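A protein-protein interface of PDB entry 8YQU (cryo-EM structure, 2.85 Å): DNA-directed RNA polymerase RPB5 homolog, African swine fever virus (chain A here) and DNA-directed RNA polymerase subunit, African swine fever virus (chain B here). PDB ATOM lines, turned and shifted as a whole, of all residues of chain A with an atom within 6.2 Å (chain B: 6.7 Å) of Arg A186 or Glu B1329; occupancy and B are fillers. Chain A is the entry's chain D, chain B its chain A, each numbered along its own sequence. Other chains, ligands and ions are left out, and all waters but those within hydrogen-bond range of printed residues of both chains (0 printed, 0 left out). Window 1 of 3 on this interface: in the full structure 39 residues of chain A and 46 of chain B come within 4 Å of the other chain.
The side-chain carboxylate (OE2) of Glu B857 is in salt-bridge range of the guanidinium group (NH2) of Arg A186 (3.1 Å). N of Ile B1328 is in hydrogen-bond range of OD1 of Asp A168, at 3.0 Å. OE1 of Glu B1329 is in salt-bridge range of NH1 of Arg A186 (3.4 Å). The guanidinium group (NE) of Arg A198 lies within salt-bridge range of the side-chain carboxylate (OE2) of Glu B1329. The guanidinium group of Arg A186 is in salt-bridge range of the side-chain carboxylate of Asp B1358 (3.7 Å). The backbone carbonyl oxygen (O) of Thr B1361 lies within hydrogen-bond range of the guanidinium group (NH2) of Arg A198, at 2.8 Å. NE of Arg B1332 sits close to NH1 of Arg A186 (3.4 Å). OG of Ser A188 lies close to OE1 of Glu B857 (2.4 Å).
The side-chain amide nitrogen of Gln B852 is in hydrogen-bond range of the side-chain carboxylate of Asp B1358, 2.5 Å away. The side-chain sulfur of Met B1323 lies close to the backbone NH of Ile B1328 (3.6 Å). The guanidinium group of Arg B1332 lies close to the side-chain amide nitrogen of Gln B1333. The guanidinium group (NH1) of Arg B1332 lies within salt-bridge range of the side-chain carboxylate (OD1) of Asp B1358 (2.6 Å). The backbone NH of Ile A184 is in hydrogen-bond range of the backbone carbonyl oxygen of Val A196, at 2.9 Å. O of Arg A186 is in hydrogen-bond range of N of Ala A194 (2.9 Å).
Among the printed residues, pairs that only touch across the chains: Asp A168 with Gly B1327 (3.1 Å), Met A192 with Ile B911 (3.1 Å), Ile A184 with Glu B1329 (3.3 Å), His A139 with Glu B1329 (3.4 Å), Ala A135 with Ala B1330 (3.4 Å), Pro A187 with Gln B1333 (3.5 Å), Ile A136 with Tyr B1326 (3.6 Å), Pro A137 with Glu B1329 (3.6 Å), Ala A194 with Glu B857 (3.6 Å), Ile A164 with Ile B1328 (3.7 Å), His A193 with Ile B911 (3.8 Å), Met A162 with Val B851 (3.9 Å) and Pro A187 with Ile B911 (3.99 Å).
Arg A186 touches four residues of chain B. Of chain A, only Pro A137, His A139, Ile A184, Arg A186 and Arg A198 come within 4 Å of Glu B1329. Of the printed residues of chain A, Gln B1333 touches Pro A187 (3.5 Å). Printed residues of chain B within 4 Å of Ile A136: Tyr B1326. Met B1323 touches none of the printed residues of chain A. Val A196 touches none of the printed residues of chain B. The nearest residue of chain B that does not touch Arg A186 is Gln B1333 (5.1 Å). The nearest residue of chain A that does not touch Glu B1329 is Val A196 (4.4 Å).
Of the 18 printed residues of chain B, 12 touch a printed residue of chain A. Of the 19 printed residues of chain A, 15 touch a printed residue of chain B. Printed residues of chain A that touch a printed residue of chain B: Ala A135, Ile A136, Pro A137, His A139, Met A162, Ile A164, Asp A168, Ile A184, Arg A186, Pro A187, Ser A188, Met A192, His A193, Ala A194 and Arg A198. Among the printed residues, 21 pairs touch across the chains.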
ATOM      1  N   ALA A 135      23.317   5.560 -10.113  1.00  0.00           N
ATOM      2  CA  ALA A 135      22.082   5.186  -9.435  1.00  0.00           C
ATOM      3  C   ALA A 135      21.026   6.281  -9.458  1.00  0.00           C
ATOM      4  O   ALA A 135      19.884   6.019  -9.072  1.00  0.00           O
ATOM      5  CB  ALA A 135      22.379   4.795  -7.987  1.00  0.00           C
ATOM      6  N   ILE A 136      21.370   7.487  -9.893  1.00  0.00           N
ATOM      7  CA  ILE A 136      20.478   8.640  -9.824  1.00  0.00           C
ATOM      8  C   ILE A 136      19.889   8.878 -11.211  1.00  0.00           C
ATOM      9  O   ILE A 136      20.652   9.119 -12.159  1.00  0.00           O
ATOM     10  CB  ILE A 136      21.213   9.885  -9.311  1.00  0.00           C
ATOM     11  CG1 ILE A 136      21.490   9.738  -7.815  1.00  0.00           C
ATOM     12  CG2 ILE A 136      20.401  11.139  -9.584  1.00  0.00           C
ATOM     13  CD1 ILE A 136      22.425  10.769  -7.263  1.00  0.00           C
ATOM     14  N   PRO A 137      18.561   8.814 -11.378  1.00  0.00           N
ATOM     15  CA  PRO A 137      17.955   9.078 -12.692  1.00  0.00           C
ATOM     16  C   PRO A 137      18.164  10.510 -13.158  1.00  0.00           C
ATOM     17  O   PRO A 137      18.769  11.317 -12.446  1.00  0.00           O
ATOM     18  CB  PRO A 137      16.469   8.784 -12.458  1.00  0.00           C
ATOM     19  CG  PRO A 137      16.435   7.894 -11.266  1.00  0.00           C
ATOM     20  CD  PRO A 137      17.573   8.331 -10.400  1.00  0.00           C
ATOM     21  N   LYS A 138      17.664  10.845 -14.346  1.00  0.00           N
ATOM     22  CA  LYS A 138      17.883  12.169 -14.919  1.00  0.00           C
ATOM     23  C   LYS A 138      16.732  13.089 -14.525  1.00  0.00           C
ATOM     24  O   LYS A 138      15.592  12.893 -14.958  1.00  0.00           O
ATOM     25  CB  LYS A 138      18.033  12.084 -16.434  1.00  0.00           C
ATOM     26  CG  LYS A 138      19.230  11.262 -16.869  1.00  0.00           C
ATOM     27  CD  LYS A 138      20.526  11.948 -16.463  1.00  0.00           C
ATOM     28  CE  LYS A 138      21.742  11.179 -16.947  1.00  0.00           C
ATOM     29  NZ  LYS A 138      23.010  11.826 -16.508  1.00  0.00           N
ATOM     30  N   HIS A 139      17.035  14.094 -13.709  1.00  0.00           N
ATOM     31  CA  HIS A 139      16.063  15.093 -13.299  1.00  0.00           C
ATOM     32  C   HIS A 139      16.178  16.329 -14.185  1.00  0.00           C
ATOM     33  O   HIS A 139      17.256  16.657 -14.685  1.00  0.00           O
ATOM     34  CB  HIS A 139      16.276  15.483 -11.835  1.00  0.00           C
ATOM     35  CG  HIS A 139      16.097  14.354 -10.870  1.00  0.00           C
ATOM     36  ND1 HIS A 139      16.928  13.254 -10.847  1.00  0.00           N
ATOM     37  CD2 HIS A 139      15.192  14.162  -9.883  1.00  0.00           C
ATOM     38  CE1 HIS A 139      16.536  12.429  -9.893  1.00  0.00           C
ATOM     39  NE2 HIS A 139      15.485  12.956  -9.292  1.00  0.00           N
ATOM     40  N   MET A 162       3.276  12.987  -7.290  1.00  0.00           N
ATOM     41  CA  MET A 162       4.321  12.652  -6.337  1.00  0.00           C
ATOM     42  C   MET A 162       5.100  13.912  -5.983  1.00  0.00           C
ATOM     43  O   MET A 162       5.212  14.843  -6.783  1.00  0.00           O
ATOM     44  CB  MET A 162       5.268  11.595  -6.907  1.00  0.00           C
ATOM     45  CG  MET A 162       4.718  10.180  -6.909  1.00  0.00           C
ATOM     46  SD  MET A 162       3.490   9.905  -8.196  1.00  0.00           S
ATOM     47  CE  MET A 162       4.539   9.823  -9.644  1.00  0.00           C
ATOM     48  N   ILE A 164       8.636  15.713  -4.098  1.00  0.00           N
ATOM     49  CA  ILE A 164      10.052  15.547  -3.803  1.00  0.00           C
ATOM     50  C   ILE A 164      10.534  16.780  -3.049  1.00  0.00           C
ATOM     51  O   ILE A 164      10.143  17.908  -3.368  1.00  0.00           O
ATOM     52  CB  ILE A 164      10.874  15.315  -5.092  1.00  0.00           C
ATOM     53  CG1 ILE A 164      12.323  14.956  -4.764  1.00  0.00           C
ATOM     54  CG2 ILE A 164      10.800  16.519  -6.023  1.00  0.00           C
ATOM     55  CD1 ILE A 164      13.067  14.344  -5.929  1.00  0.00           C
ATOM     56  N   ASP A 168      16.505  17.515  -1.795  1.00  0.00           N
ATOM     57  CA  ASP A 168      16.928  16.300  -2.470  1.00  0.00           C
ATOM     58  C   ASP A 168      18.143  16.604  -3.346  1.00  0.00           C
ATOM     59  O   ASP A 168      18.146  17.606  -4.072  1.00  0.00           O
ATOM     60  CB  ASP A 168      15.767  15.751  -3.302  1.00  0.00           C
ATOM     61  CG  ASP A 168      16.050  14.392  -3.893  1.00  0.00           C
ATOM     62  OD1 ASP A 168      16.038  13.407  -3.129  1.00  0.00           O
ATOM     63  OD2 ASP A 168      16.238  14.299  -5.120  1.00  0.00           O
ATOM     64  N   ILE A 184      11.385  13.579 -14.222  1.00  0.00           N
ATOM     65  CA  ILE A 184      12.428  12.590 -13.990  1.00  0.00           C
ATOM     66  C   ILE A 184      12.285  11.496 -15.036  1.00  0.00           C
ATOM     67  O   ILE A 184      11.232  10.851 -15.134  1.00  0.00           O
ATOM     68  CB  ILE A 184      12.349  12.007 -12.573  1.00  0.00           C
ATOM     69  CG1 ILE A 184      12.330  13.131 -11.539  1.00  0.00           C
ATOM     70  CG2 ILE A 184      13.508  11.058 -12.325  1.00  0.00           C
ATOM     71  CD1 ILE A 184      11.907  12.683 -10.167  1.00  0.00           C
ATOM     72  N   GLU A 185      13.342  11.295 -15.816  1.00  0.00           N
ATOM     73  CA  GLU A 185      13.454  10.160 -16.717  1.00  0.00           C
ATOM     74  C   GLU A 185      14.311   9.108 -16.027  1.00  0.00           C
ATOM     75  O   GLU A 185      15.467   9.376 -15.673  1.00  0.00           O
ATOM     76  CB  GLU A 185      14.060  10.574 -18.057  1.00  0.00           C
ATOM     77  CG  GLU A 185      13.228  11.597 -18.809  1.00  0.00           C
ATOM     78  CD  GLU A 185      13.348  11.461 -20.313  1.00  0.00           C
ATOM     79  OE1 GLU A 185      14.079  10.559 -20.774  1.00  0.00           O
ATOM     80  OE2 GLU A 185      12.708  12.255 -21.034  1.00  0.00           O
ATOM     81  N   ARG A 186      13.740   7.927 -15.823  1.00  0.00           N
ATOM     82  CA  ARG A 186      14.369   6.908 -15.003  1.00  0.00           C
ATOM     83  C   ARG A 186      14.351   5.560 -15.706  1.00  0.00           C
ATOM     84  O   ARG A 186      13.448   5.277 -16.500  1.00  0.00           O
ATOM     85  CB  ARG A 186      13.661   6.797 -13.644  1.00  0.00           C
ATOM     86  CG  ARG A 186      12.187   6.432 -13.714  1.00  0.00           C
ATOM     87  CD  ARG A 186      11.497   6.802 -12.411  1.00  0.00           C
ATOM     88  NE  ARG A 186      10.183   6.188 -12.263  1.00  0.00           N
ATOM     89  CZ  ARG A 186       9.376   6.399 -11.233  1.00  0.00           C
ATOM     90  NH1 ARG A 186       9.714   7.210 -10.245  1.00  0.00           N
ATOM     91  NH2 ARG A 186       8.198   5.782 -11.195  1.00  0.00           N
ATOM     92  N   PRO A 187      15.345   4.716 -15.441  1.00  0.00           N
ATOM     93  CA  PRO A 187      15.373   3.389 -16.061  1.00  0.00           C
ATOM     94  C   PRO A 187      14.242   2.513 -15.550  1.00  0.00           C
ATOM     95  O   PRO A 187      13.730   2.684 -14.442  1.00  0.00           O
ATOM     96  CB  PRO A 187      16.739   2.827 -15.646  1.00  0.00           C
ATOM     97  CG  PRO A 187      17.534   4.021 -15.211  1.00  0.00           C
ATOM     98  CD  PRO A 187      16.537   4.956 -14.615  1.00  0.00           C
ATOM     99  N   SER A 188      13.851   1.557 -16.388  1.00  0.00           N
ATOM    100  CA  SER A 188      12.777   0.639 -16.048  1.00  0.00           C
ATOM    101  C   SER A 188      13.108  -0.736 -16.600  1.00  0.00           C
ATOM    102  O   SER A 188      13.711  -0.854 -17.670  1.00  0.00           O
ATOM    103  CB  SER A 188      11.433   1.123 -16.601  1.00  0.00           C
ATOM    104  OG  SER A 188      10.360   0.372 -16.061  1.00  0.00           O
ATOM    105  N   MET A 192      11.614  -0.335 -20.271  1.00  0.00           N
ATOM    106  CA  MET A 192      12.983   0.033 -20.627  1.00  0.00           C
ATOM    107  C   MET A 192      13.322   1.461 -20.206  1.00  0.00           C
ATOM    108  O   MET A 192      14.499   1.822 -20.147  1.00  0.00           O
ATOM    109  CB  MET A 192      13.210  -0.155 -22.134  1.00  0.00           C
ATOM    110  CG  MET A 192      14.622   0.131 -22.624  1.00  0.00           C
ATOM    111  SD  MET A 192      14.824  -0.131 -24.395  1.00  0.00           S
ATOM    112  CE  MET A 192      13.922   1.266 -25.054  1.00  0.00           C
ATOM    113  N   HIS A 193      12.313   2.252 -19.847  1.00  0.00           N
ATOM    114  CA  HIS A 193      12.474   3.553 -19.200  1.00  0.00           C
ATOM    115  C   HIS A 193      11.091   4.151 -18.984  1.00  0.00           C
ATOM    116  O   HIS A 193      10.117   3.752 -19.626  1.00  0.00           O
ATOM    117  CB  HIS A 193      13.363   4.527 -19.992  1.00  0.00           C
ATOM    118  CG  HIS A 193      12.954   4.719 -21.418  1.00  0.00           C
ATOM    119  ND1 HIS A 193      12.980   3.701 -22.347  1.00  0.00           N
ATOM    120  CD2 HIS A 193      12.546   5.824 -22.085  1.00  0.00           C
ATOM    121  CE1 HIS A 193      12.586   4.166 -23.518  1.00  0.00           C
ATOM    122  NE2 HIS A 193      12.315   5.451 -23.387  1.00  0.00           N
ATOM    123  N   ALA A 194      11.025   5.120 -18.074  1.00  0.00           N
ATOM    124  CA  ALA A 194       9.771   5.768 -17.723  1.00  0.00           C
ATOM    125  C   ALA A 194      10.027   7.237 -17.425  1.00  0.00           C
ATOM    126  O   ALA A 194      11.159   7.655 -17.163  1.00  0.00           O
ATOM    127  CB  ALA A 194       9.104   5.092 -16.521  1.00  0.00           C
ATOM    128  N   VAL A 195       8.953   8.019 -17.476  1.00  0.00           N
ATOM    129  CA  VAL A 195       8.996   9.455 -17.223  1.00  0.00           C
ATOM    130  C   VAL A 195       7.928   9.786 -16.194  1.00  0.00           C
ATOM    131  O   VAL A 195       6.756   9.439 -16.379  1.00  0.00           O
ATOM    132  CB  VAL A 195       8.777  10.271 -18.507  1.00  0.00           C
ATOM    133  CG1 VAL A 195       8.515  11.726 -18.170  1.00  0.00           C
ATOM    134  CG2 VAL A 195       9.977  10.144 -19.423  1.00  0.00           C
ATOM    135  N   VAL A 196       8.327  10.455 -15.114  1.00  0.00           N
ATOM    136  CA  VAL A 196       7.400  10.902 -14.086  1.00  0.00           C
ATOM    137  C   VAL A 196       7.603  12.397 -13.869  1.00  0.00           C
ATOM    138  O   VAL A 196       8.589  12.984 -14.308  1.00  0.00           O
ATOM    139  CB  VAL A 196       7.566  10.130 -12.764  1.00  0.00           C
ATOM    140  CG1 VAL A 196       7.276   8.654 -12.973  1.00  0.00           C
ATOM    141  CG2 VAL A 196       8.961  10.332 -12.203  1.00  0.00           C
ATOM    142  N   ARG A 198       7.287  15.268 -10.640  1.00  0.00           N
ATOM    143  CA  ARG A 198       7.183  15.427  -9.200  1.00  0.00           C
ATOM    144  C   ARG A 198       7.084  16.903  -8.839  1.00  0.00           C
ATOM    145  O   ARG A 198       7.657  17.768  -9.511  1.00  0.00           O
ATOM    146  CB  ARG A 198       8.381  14.795  -8.484  1.00  0.00           C
ATOM    147  CG  ARG A 198       8.279  13.290  -8.320  1.00  0.00           C
ATOM    148  CD  ARG A 198       9.457  12.751  -7.532  1.00  0.00           C
ATOM    149  NE  ARG A 198       9.323  11.329  -7.245  1.00  0.00           N
ATOM    150  CZ  ARG A 198       8.982  10.833  -6.064  1.00  0.00           C
ATOM    151  NH1 ARG A 198       8.724  11.620  -5.033  1.00  0.00           N
ATOM    152  NH2 ARG A 198       8.899   9.514  -5.913  1.00  0.00           N
ATOM    153  N   VAL B 851       0.280   7.448  -7.161  1.00  0.00           N
ATOM    154  CA  VAL B 851       1.365   6.595  -6.704  1.00  0.00           C
ATOM    155  C   VAL B 851       2.240   6.153  -7.869  1.00  0.00           C
ATOM    156  O   VAL B 851       3.459   6.042  -7.732  1.00  0.00           O
ATOM    157  CB  VAL B 851       0.799   5.383  -5.933  1.00  0.00           C
ATOM    158  CG1 VAL B 851       1.877   4.344  -5.681  1.00  0.00           C
ATOM    159  CG2 VAL B 851       0.180   5.834  -4.625  1.00  0.00           C
ATOM    160  N   GLN B 852       1.626   5.925  -9.027  1.00  0.00           N
ATOM    161  CA  GLN B 852       2.335   5.616 -10.256  1.00  0.00           C
ATOM    162  C   GLN B 852       1.695   6.385 -11.400  1.00  0.00           C
ATOM    163  O   GLN B 852       0.467   6.465 -11.491  1.00  0.00           O
ATOM    164  CB  GLN B 852       2.304   4.114 -10.558  1.00  0.00           C
ATOM    165  CG  GLN B 852       3.286   3.306  -9.742  1.00  0.00           C
ATOM    166  CD  GLN B 852       3.243   1.831 -10.068  1.00  0.00           C
ATOM    167  OE1 GLN B 852       2.321   1.356 -10.727  1.00  0.00           O
ATOM    168  NE2 GLN B 852       4.248   1.094  -9.613  1.00  0.00           N
ATOM    169  N   GLN B 853       2.531   6.955 -12.269  1.00  0.00           N
ATOM    170  CA  GLN B 853       2.008   7.609 -13.463  1.00  0.00           C
ATOM    171  C   GLN B 853       1.415   6.593 -14.430  1.00  0.00           C
ATOM    172  O   GLN B 853       0.506   6.923 -15.199  1.00  0.00           O
ATOM    173  CB  GLN B 853       3.111   8.419 -14.143  1.00  0.00           C
ATOM    174  CG  GLN B 853       2.619   9.328 -15.251  1.00  0.00           C
ATOM    175  CD  GLN B 853       1.955  10.581 -14.720  1.00  0.00           C
ATOM    176  OE1 GLN B 853       2.515  11.283 -13.879  1.00  0.00           O
ATOM    177  NE2 GLN B 853       0.756  10.866 -15.207  1.00  0.00           N
ATOM    178  N   GLU B 857       4.775   1.022 -14.998  1.00  0.00           N
ATOM    179  CA  GLU B 857       5.463   1.846 -15.987  1.00  0.00           C
ATOM    180  C   GLU B 857       5.259   1.351 -17.413  1.00  0.00           C
ATOM    181  O   GLU B 857       5.866   1.892 -18.345  1.00  0.00           O
ATOM    182  CB  GLU B 857       6.958   1.973 -15.672  1.00  0.00           C
ATOM    183  CG  GLU B 857       7.235   2.799 -14.425  1.00  0.00           C
ATOM    184  CD  GLU B 857       8.615   2.562 -13.854  1.00  0.00           C
ATOM    185  OE1 GLU B 857       9.319   1.659 -14.348  1.00  0.00           O
ATOM    186  OE2 GLU B 857       8.996   3.279 -12.905  1.00  0.00           O
ATOM    187  N   ILE B 911      20.745   1.955 -21.243  1.00  0.00           N
ATOM    188  CA  ILE B 911      19.870   1.955 -20.075  1.00  0.00           C
ATOM    189  C   ILE B 911      20.158   0.753 -19.183  1.00  0.00           C
ATOM    190  O   ILE B 911      20.304   0.887 -17.963  1.00  0.00           O
ATOM    191  CB  ILE B 911      18.396   1.993 -20.511  1.00  0.00           C
ATOM    192  CG1 ILE B 911      18.032   3.388 -21.020  1.00  0.00           C
ATOM    193  CG2 ILE B 911      17.497   1.589 -19.359  1.00  0.00           C
ATOM    194  CD1 ILE B 911      16.744   3.436 -21.803  1.00  0.00           C
ATOM    195  N   MET B1323      19.227   6.711   0.473  1.00  0.00           N
ATOM    196  CA  MET B1323      18.317   7.851   0.515  1.00  0.00           C
ATOM    197  C   MET B1323      19.022   9.107   1.011  1.00  0.00           C
ATOM    198  O   MET B1323      18.785  10.206   0.496  1.00  0.00           O
ATOM    199  CB  MET B1323      17.117   7.523   1.404  1.00  0.00           C
ATOM    200  CG  MET B1323      16.203   8.698   1.695  1.00  0.00           C
ATOM    201  SD  MET B1323      15.459   9.409   0.221  1.00  0.00           S
ATOM    202  CE  MET B1323      14.952  11.009   0.841  1.00  0.00           C
ATOM    203  N   TYR B1326      21.940  10.021  -1.985  1.00  0.00           N
ATOM    204  CA  TYR B1326      21.598  10.055  -3.402  1.00  0.00           C
ATOM    205  C   TYR B1326      20.230  10.648  -3.689  1.00  0.00           C
ATOM    206  O   TYR B1326      20.083  11.393  -4.660  1.00  0.00           O
ATOM    207  CB  TYR B1326      21.676   8.645  -3.995  1.00  0.00           C
ATOM    208  CG  TYR B1326      23.081   8.093  -4.061  1.00  0.00           C
ATOM    209  CD1 TYR B1326      24.167   8.931  -4.269  1.00  0.00           C
ATOM    210  CD2 TYR B1326      23.322   6.734  -3.916  1.00  0.00           C
ATOM    211  CE1 TYR B1326      25.451   8.434  -4.330  1.00  0.00           C
ATOM    212  CE2 TYR B1326      24.604   6.227  -3.975  1.00  0.00           C
ATOM    213  CZ  TYR B1326      25.665   7.080  -4.182  1.00  0.00           C
ATOM    214  OH  TYR B1326      26.944   6.580  -4.243  1.00  0.00           O
ATOM    215  N   GLY B1327      19.221  10.346  -2.879  1.00  0.00           N
ATOM    216  CA  GLY B1327      17.921  10.958  -3.032  1.00  0.00           C
ATOM    217  C   GLY B1327      16.812   9.936  -2.975  1.00  0.00           C
ATOM    218  O   GLY B1327      17.027   8.759  -2.670  1.00  0.00           O
ATOM    219  N   ILE B1328      15.597  10.395  -3.279  1.00  0.00           N
ATOM    220  CA  ILE B1328      14.433   9.519  -3.201  1.00  0.00           C
ATOM    221  C   ILE B1328      14.308   8.648  -4.447  1.00  0.00           C
ATOM    222  O   ILE B1328      13.792   7.527  -4.373  1.00  0.00           O
ATOM    223  CB  ILE B1328      13.156  10.345  -2.958  1.00  0.00           C
ATOM    224  CG1 ILE B1328      12.005   9.439  -2.520  1.00  0.00           C
ATOM    225  CG2 ILE B1328      12.770  11.138  -4.196  1.00  0.00           C
ATOM    226  CD1 ILE B1328      12.285   8.671  -1.254  1.00  0.00           C
ATOM    227  N   GLU B1329      14.774   9.131  -5.601  1.00  0.00           N
ATOM    228  CA  GLU B1329      14.705   8.321  -6.813  1.00  0.00           C
ATOM    229  C   GLU B1329      15.674   7.150  -6.751  1.00  0.00           C
ATOM    230  O   GLU B1329      15.336   6.035  -7.162  1.00  0.00           O
ATOM    231  CB  GLU B1329      14.979   9.187  -8.039  1.00  0.00           C
ATOM    232  CG  GLU B1329      13.831  10.107  -8.401  1.00  0.00           C
ATOM    233  CD  GLU B1329      12.647   9.351  -8.967  1.00  0.00           C
ATOM    234  OE1 GLU B1329      12.867   8.383  -9.722  1.00  0.00           O
ATOM    235  OE2 GLU B1329      11.497   9.723  -8.654  1.00  0.00           O
ATOM    236  N   ALA B1330      16.885   7.381  -6.240  1.00  0.00           N
ATOM    237  CA  ALA B1330      17.821   6.278  -6.057  1.00  0.00           C
ATOM    238  C   ALA B1330      17.386   5.363  -4.922  1.00  0.00           C
ATOM    239  O   ALA B1330      17.655   4.157  -4.963  1.00  0.00           O
ATOM    240  CB  ALA B1330      19.226   6.815  -5.799  1.00  0.00           C
ATOM    241  N   ALA B1331      16.714   5.912  -3.907  1.00  0.00           N
ATOM    242  CA  ALA B1331      16.154   5.070  -2.858  1.00  0.00           C
ATOM    243  C   ALA B1331      14.999   4.229  -3.381  1.00  0.00           C
ATOM    244  O   ALA B1331      14.763   3.122  -2.883  1.00  0.00           O
ATOM    245  CB  ALA B1331      15.695   5.928  -1.680  1.00  0.00           C
ATOM    246  N   ARG B1332      14.267   4.738  -4.375  1.00  0.00           N
ATOM    247  CA  ARG B1332      13.217   3.945  -5.003  1.00  0.00           C
ATOM    248  C   ARG B1332      13.796   2.724  -5.702  1.00  0.00           C
ATOM    249  O   ARG B1332      13.266   1.615  -5.574  1.00  0.00           O
ATOM    250  CB  ARG B1332      12.440   4.806  -5.996  1.00  0.00           C
ATOM    251  CG  ARG B1332      11.108   4.225  -6.407  1.00  0.00           C
ATOM    252  CD  ARG B1332      10.545   4.969  -7.598  1.00  0.00           C
ATOM    253  NE  ARG B1332      11.171   4.537  -8.841  1.00  0.00           N
ATOM    254  CZ  ARG B1332      10.749   3.516  -9.573  1.00  0.00           C
ATOM    255  NH1 ARG B1332       9.695   2.801  -9.218  1.00  0.00           N
ATOM    256  NH2 ARG B1332      11.400   3.204 -10.690  1.00  0.00           N
ATOM    257  N   GLN B1333      14.887   2.909  -6.448  1.00  0.00           N
ATOM    258  CA  GLN B1333      15.542   1.783  -7.102  1.00  0.00           C
ATOM    259  C   GLN B1333      16.193   0.848  -6.091  1.00  0.00           C
ATOM    260  O   GLN B1333      16.398  -0.335  -6.384  1.00  0.00           O
ATOM    261  CB  GLN B1333      16.585   2.287  -8.098  1.00  0.00           C
ATOM    262  CG  GLN B1333      16.004   2.939  -9.340  1.00  0.00           C
ATOM    263  CD  GLN B1333      15.293   1.949 -10.237  1.00  0.00           C
ATOM    264  OE1 GLN B1333      15.617   0.763 -10.252  1.00  0.00           O
ATOM    265  NE2 GLN B1333      14.319   2.434 -10.997  1.00  0.00           N
ATOM    266  N   LYS B1334      16.530   1.357  -4.906  1.00  0.00           N
ATOM    267  CA  LYS B1334      17.156   0.521  -3.889  1.00  0.00           C
ATOM    268  C   LYS B1334      16.145  -0.405  -3.227  1.00  0.00           C
ATOM    269  O   LYS B1334      16.470  -1.552  -2.905  1.00  0.00           O
ATOM    270  CB  LYS B1334      17.845   1.397  -2.841  1.00  0.00           C
ATOM    271  CG  LYS B1334      18.685   0.627  -1.836  1.00  0.00           C
ATOM    272  CD  LYS B1334      19.642  -0.327  -2.530  1.00  0.00           C
ATOM    273  CE  LYS B1334      20.652   0.421  -3.384  1.00  0.00           C
ATOM    274  NZ  LYS B1334      21.602  -0.511  -4.050  1.00  0.00           N
ATOM    275  N   LEU B1354       7.727  -2.580  -8.026  1.00  0.00           N
ATOM    276  CA  LEU B1354       7.513  -1.146  -8.189  1.00  0.00           C
ATOM    277  C   LEU B1354       6.412  -0.635  -7.276  1.00  0.00           C
ATOM    278  O   LEU B1354       6.488   0.497  -6.788  1.00  0.00           O
ATOM    279  CB  LEU B1354       7.174  -0.813  -9.642  1.00  0.00           C
ATOM    280  CG  LEU B1354       8.299  -0.709 -10.670  1.00  0.00           C
ATOM    281  CD1 LEU B1354       8.895  -2.052 -10.975  1.00  0.00           C
ATOM    282  CD2 LEU B1354       7.760  -0.084 -11.937  1.00  0.00           C
ATOM    283  N   ASP B1358       7.156   2.512  -5.136  1.00  0.00           N
ATOM    284  CA  ASP B1358       6.442   3.729  -5.508  1.00  0.00           C
ATOM    285  C   ASP B1358       5.534   4.214  -4.388  1.00  0.00           C
ATOM    286  O   ASP B1358       5.380   5.425  -4.198  1.00  0.00           O
ATOM    287  CB  ASP B1358       5.640   3.490  -6.785  1.00  0.00           C
ATOM    288  CG  ASP B1358       6.528   3.313  -7.998  1.00  0.00           C
ATOM    289  OD1 ASP B1358       7.628   3.899  -8.015  1.00  0.00           O
ATOM    290  OD2 ASP B1358       6.148   2.566  -8.921  1.00  0.00           O
ATOM    291  N   THR B1361       7.772   5.696  -1.444  1.00  0.00           N
ATOM    292  CA  THR B1361       8.594   6.848  -1.797  1.00  0.00           C
ATOM    293  C   THR B1361       7.798   7.930  -2.519  1.00  0.00           C
ATOM    294  O   THR B1361       8.388   8.757  -3.219  1.00  0.00           O
ATOM    295  CB  THR B1361       9.780   6.419  -2.662  1.00  0.00           C
ATOM    296  OG1 THR B1361       9.298   5.815  -3.868  1.00  0.00           O
ATOM    297  CG2 THR B1361      10.652   5.421  -1.921  1.00  0.00           C
